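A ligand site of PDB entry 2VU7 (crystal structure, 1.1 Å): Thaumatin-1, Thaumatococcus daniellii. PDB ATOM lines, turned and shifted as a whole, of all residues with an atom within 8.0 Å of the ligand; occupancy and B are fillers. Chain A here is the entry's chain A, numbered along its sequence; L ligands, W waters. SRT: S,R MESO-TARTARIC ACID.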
ATOM      1  N   TRP A  51       4.285   6.196  18.271  1.00  0.00           N
ATOM      2  CA  TRP A  51       4.095   5.170  17.255  1.00  0.00           C
ATOM      3  C   TRP A  51       5.231   4.167  17.330  1.00  0.00           C
ATOM      4  O   TRP A  51       6.267   4.404  17.953  1.00  0.00           O
ATOM      5  CB  TRP A  51       3.967   5.790  15.843  1.00  0.00           C
ATOM      6  CG  TRP A  51       5.185   6.468  15.306  1.00  0.00           C
ATOM      7  CD1 TRP A  51       6.012   6.010  14.327  1.00  0.00           C
ATOM      8  CD2 TRP A  51       5.653   7.804  15.604  1.00  0.00           C
ATOM      9  NE1 TRP A  51       6.986   6.936  14.007  1.00  0.00           N
ATOM     10  CE2 TRP A  51       6.793   8.041  14.790  1.00  0.00           C
ATOM     11  CE3 TRP A  51       5.240   8.808  16.507  1.00  0.00           C
ATOM     12  CZ2 TRP A  51       7.507   9.259  14.847  1.00  0.00           C
ATOM     13  CZ3 TRP A  51       5.977   9.987  16.555  1.00  0.00           C
ATOM     14  CH2 TRP A  51       7.094  10.192  15.751  1.00  0.00           C
ATOM     15  N   CYS A  66      14.149   3.368   8.840  1.00  0.00           N
ATOM     16  CA  CYS A  66      13.077   2.437   9.153  1.00  0.00           C
ATOM     17  C   CYS A  66      12.167   2.239   7.949  1.00  0.00           C
ATOM     18  O   CYS A  66      11.887   3.180   7.214  1.00  0.00           O
ATOM     19  CB  CYS A  66      12.207   2.974  10.289  1.00  0.00           C
ATOM     20  SG  CYS A  66      13.113   3.122  11.856  1.00  0.00           S
ATOM     21  N   GLY A  69       7.334   4.373   9.482  1.00  0.00           N
ATOM     22  CA  GLY A  69       7.441   5.370  10.533  1.00  0.00           C
ATOM     23  C   GLY A  69       8.756   6.111  10.687  1.00  0.00           C
ATOM     24  O   GLY A  69       8.968   6.747  11.731  1.00  0.00           O
ATOM     25  N   ASP A  70       9.613   6.059   9.664  1.00  0.00           N
ATOM     26  CA  ASP A  70      10.908   6.730   9.750  1.00  0.00           C
ATOM     27  C   ASP A  70      10.726   8.220  10.044  1.00  0.00           C
ATOM     28  O   ASP A  70       9.898   8.884   9.434  1.00  0.00           O
ATOM     29  CB  ASP A  70      11.674   6.550   8.450  1.00  0.00           C
ATOM     30  CG  ASP A  70      13.107   7.002   8.592  1.00  0.00           C
ATOM     31  OD1 ASP A  70      13.887   6.276   9.268  1.00  0.00           O
ATOM     32  OD2 ASP A  70      13.407   8.103   8.071  1.00  0.00           O
ATOM     33  N   CYS A  71      11.555   8.738  10.972  1.00  0.00           N
ATOM     34  CA  CYS A  71      11.518  10.152  11.323  1.00  0.00           C
ATOM     35  C   CYS A  71      12.839  10.799  10.968  1.00  0.00           C
ATOM     36  O   CYS A  71      13.732  10.944  11.821  1.00  0.00           O
ATOM     37  CB  CYS A  71      11.166  10.334  12.816  1.00  0.00           C
ATOM     38  SG  CYS A  71      12.452   9.550  13.895  1.00  0.00           S
ATOM     39  N   GLY A  72      12.985  11.175   9.709  1.00  0.00           N
ATOM     40  CA  GLY A  72      14.196  11.905   9.316  1.00  0.00           C
ATOM     41  C   GLY A  72      15.463  11.073   9.518  1.00  0.00           C
ATOM     42  O   GLY A  72      16.527  11.652   9.719  1.00  0.00           O
ATOM     43  N   GLY A  73      15.360   9.741   9.500  1.00  0.00           N
ATOM     44  CA  GLY A  73      16.543   8.919   9.599  1.00  0.00           C
ATOM     45  C   GLY A  73      17.157   8.901  10.996  1.00  0.00           C
ATOM     46  O   GLY A  73      18.326   8.485  11.130  1.00  0.00           O
ATOM     47  N   LEU A  74      16.390   9.270  12.021  1.00  0.00           N
ATOM     48  CA  LEU A  74      16.916   9.309  13.392  1.00  0.00           C
ATOM     49  C   LEU A  74      16.341   8.219  14.241  1.00  0.00           C
ATOM     50  O   LEU A  74      15.159   7.876  14.133  1.00  0.00           O
ATOM     51  CB  LEU A  74      16.618  10.642  14.057  1.00  0.00           C
ATOM     52  CG  LEU A  74      17.177  11.866  13.380  1.00  0.00           C
ATOM     53  CD1 LEU A  74      16.858  13.112  14.240  1.00  0.00           C
ATOM     54  CD2 LEU A  74      18.701  11.705  13.203  1.00  0.00           C
ATOM     55  N   CYS A  77      13.546  10.356  17.600  1.00  0.00           N
ATOM     56  CA  CYS A  77      12.711  11.190  16.733  1.00  0.00           C
ATOM     57  C   CYS A  77      12.434  12.559  17.307  1.00  0.00           C
ATOM     58  O   CYS A  77      12.113  12.709  18.498  1.00  0.00           O
ATOM     59  CB  CYS A  77      11.338  10.542  16.466  1.00  0.00           C
ATOM     60  SG  CYS A  77      11.412   8.993  15.544  1.00  0.00           S
ATOM     61  N   LYS A  78      12.533  13.538  16.414  1.00  0.00           N
ATOM     62  CA  LYS A  78      12.170  14.933  16.713  1.00  0.00           C
ATOM     63  C   LYS A  78      10.913  15.327  16.007  1.00  0.00           C
ATOM     64  O   LYS A  78      10.353  16.307  16.385  1.00  0.00           O
ATOM     65  CB  LYS A  78      13.337  15.896  16.281  1.00  0.00           C
ATOM     66  CG  LYS A  78      14.652  15.793  16.866  1.00  0.00           C
ATOM     67  CD  LYS A  78      15.506  16.916  16.318  1.00  0.00           C
ATOM     68  CE  LYS A  78      16.119  16.719  14.946  1.00  0.00           C
ATOM     69  NZ  LYS A  78      17.306  17.638  14.788  1.00  0.00           N
ATOM     70  N   ARG A  79      10.508  14.653  14.949  1.00  0.00           N
ATOM     71  CA  ARG A  79       9.349  14.980  14.127  1.00  0.00           C
ATOM     72  C   ARG A  79       8.551  13.697  13.909  1.00  0.00           C
ATOM     73  O   ARG A  79       8.989  12.590  14.242  1.00  0.00           O
ATOM     74  CB  ARG A  79       9.747  15.692  12.820  1.00  0.00           C
ATOM     75  CG  ARG A  79      10.304  14.864  11.743  1.00  0.00           C
ATOM     76  CD  ARG A  79      10.641  15.696  10.527  1.00  0.00           C
ATOM     77  NE  ARG A  79      11.196  14.847   9.439  1.00  0.00           N
ATOM     78  CZ  ARG A  79      12.155  15.230   8.591  1.00  0.00           C
ATOM     79  NH1 ARG A  79      12.681  16.454   8.672  1.00  0.00           N
ATOM     80  NH2 ARG A  79      12.564  14.385   7.662  1.00  0.00           N
ATOM     81  N   PHE A  80       7.363  13.866  13.301  1.00  0.00           N
ATOM     82  CA  PHE A  80       6.502  12.713  13.048  1.00  0.00           C
ATOM     83  C   PHE A  80       7.074  11.844  11.934  1.00  0.00           C
ATOM     84  O   PHE A  80       7.869  12.295  11.088  1.00  0.00           O
ATOM     85  CB  PHE A  80       5.083  13.179  12.720  1.00  0.00           C
ATOM     86  CG  PHE A  80       4.404  13.903  13.845  1.00  0.00           C
ATOM     87  CD1 PHE A  80       4.544  13.478  15.147  1.00  0.00           C
ATOM     88  CD2 PHE A  80       3.596  15.016  13.595  1.00  0.00           C
ATOM     89  CE1 PHE A  80       3.910  14.159  16.183  1.00  0.00           C
ATOM     90  CE2 PHE A  80       2.937  15.685  14.640  1.00  0.00           C
ATOM     91  CZ  PHE A  80       3.100  15.253  15.944  1.00  0.00           C
ATOM     92  N   GLY A  81       6.627  10.587  11.932  1.00  0.00           N
ATOM     93  CA  GLY A  81       7.189   9.575  11.054  1.00  0.00           C
ATOM     94  C   GLY A  81       6.434   9.350   9.764  1.00  0.00           C
ATOM     95  O   GLY A  81       5.266   9.693   9.610  1.00  0.00           O
ATOM     96  N   ARG A  82       7.111   8.693   8.832  1.00  0.00           N
ATOM     97  CA  ARG A  82       6.547   8.439   7.499  1.00  0.00           C
ATOM     98  C   ARG A  82       5.471   7.358   7.594  1.00  0.00           C
ATOM     99  O   ARG A  82       5.713   6.282   8.127  1.00  0.00           O
ATOM    100  CB  ARG A  82       7.670   7.978   6.592  1.00  0.00           C
ATOM    101  CG  ARG A  82       7.273   7.788   5.144  1.00  0.00           C
ATOM    102  CD  ARG A  82       7.100   9.042   4.339  1.00  0.00           C
ATOM    103  NE  ARG A  82       8.318   9.857   4.222  1.00  0.00           N
ATOM    104  CZ  ARG A  82       9.129   9.887   3.172  1.00  0.00           C
ATOM    105  NH1 ARG A  82       8.864   9.141   2.112  1.00  0.00           N
ATOM    106  NH2 ARG A  82      10.192  10.674   3.199  1.00  0.00           N
ATOM    107  N   PRO A  83       4.279   7.619   7.005  1.00  0.00           N
ATOM    108  CA  PRO A  83       3.258   6.563   6.948  1.00  0.00           C
ATOM    109  C   PRO A  83       3.783   5.327   6.235  1.00  0.00           C
ATOM    110  O   PRO A  83       4.674   5.415   5.377  1.00  0.00           O
ATOM    111  CB  PRO A  83       2.121   7.242   6.180  1.00  0.00           C
ATOM    112  CG  PRO A  83       2.321   8.738   6.534  1.00  0.00           C
ATOM    113  CD  PRO A  83       3.784   8.914   6.480  1.00  0.00           C
ATOM    114  N   LYS A 106      -3.215   7.952   8.903  1.00  0.00           N
ATOM    115  CA  LYS A 106      -1.889   7.826   8.274  1.00  0.00           C
ATOM    116  C   LYS A 106      -1.473   6.386   8.188  1.00  0.00           C
ATOM    117  O   LYS A 106      -0.259   6.099   8.218  1.00  0.00           O
ATOM    118  CB  LYS A 106      -0.860   8.691   9.034  1.00  0.00           C
ATOM    119  CG  LYS A 106      -1.164  10.196   8.998  1.00  0.00           C
ATOM    120  CD  LYS A 106      -1.127  10.744   7.541  1.00  0.00           C
ATOM    121  CE  LYS A 106      -1.485  12.226   7.441  1.00  0.00           C
ATOM    122  NZ  LYS A 106      -1.094  12.763   6.121  1.00  0.00           N
HETATM  123  O1  SRT L   1      10.076  10.796   6.076  1.00  0.00           O
HETATM  124  O11 SRT L   1      11.553  11.691   7.401  1.00  0.00           O
HETATM  125  C1  SRT L   1      10.357  11.422   7.124  1.00  0.00           C
HETATM  126  C2  SRT L   1       9.217  11.849   8.011  1.00  0.00           C
HETATM  127  O2  SRT L   1       9.791  12.277   9.245  1.00  0.00           O
HETATM  128  C3  SRT L   1       8.468  13.048   7.370  1.00  0.00           C
HETATM  129  O3  SRT L   1       9.426  14.061   7.028  1.00  0.00           O
HETATM  130  C4  SRT L   1       7.660  12.639   6.156  1.00  0.00           C
HETATM  131  O4  SRT L   1       6.746  11.769   6.326  1.00  0.00           O
HETATM  132  O41 SRT L   1       7.920  13.166   5.038  1.00  0.00           O
HETATM  133  O   HOH W   1       4.924  12.193   8.379  1.00  0.00           O
HETATM  134  O   HOH W   2       4.772  11.771   4.445  1.00  0.00           O
HETATM  135  O   HOH W   3      13.546  11.582   5.564  1.00  0.00           O
HETATM  136  O   HOH W   4      11.866   8.818   5.792  1.00  0.00           O
HETATM  137  O   HOH W   5       8.540  16.436   6.960  1.00  0.00           O
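An oxygen (O2) of the ligand lies within hydrogen-bond range of the backbone carbonyl oxygen (O) of Phe 80 (2.7 Å).
The guanidinium group of Arg 82 lies within salt-bridge range of an oxygen (O1) of the ligand, at 2.7 Å.
N of Gly 72 lies within hydrogen-bond range of O11 of the ligand, 2.8 Å away.
NH2 of Arg 79 is in salt-bridge range of O11 of the ligand (2.9 Å).
The backbone carbonyl oxygen (O) of Asp 70 lies close to an oxygen (O2) of the ligand (3.4 Å).
The backbone NH (N) of Arg 82 sits at hydrogen-bond distance from the backbone carbonyl oxygen (O) of Asp 70 (2.9 Å).
The backbone carbonyl oxygen (O) of Arg 82 lies within hydrogen-bond range of the backbone NH (N) of Gly 69 (2.8 Å).
OD2 of Asp 70 is in hydrogen-bond range of N of Gly 73, 2.9 Å away.
The backbone NH (N) of Cys 66 sits at hydrogen-bond distance from the side-chain carboxylate (OD1) of Asp 70.
The side-chain sulfur (SG) of Cys 71 is disulfide-bonded to the side-chain sulfur (SG) of Cys 77, at 2.0 Å.
Water W4 lies within hydrogen-bond range of O1 of the ligand (2.7 Å) and OD2 of Asp 70 (2.8 Å).
Water W1 bridges O4 of the ligand (2.8 Å) and O of Gly 81 (2.8 Å).
Merely in contact with the ligand: Cys 71 (3.4 Å).
The nearest printed residue that does not touch the ligand is Pro 83 (4.1 Å).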
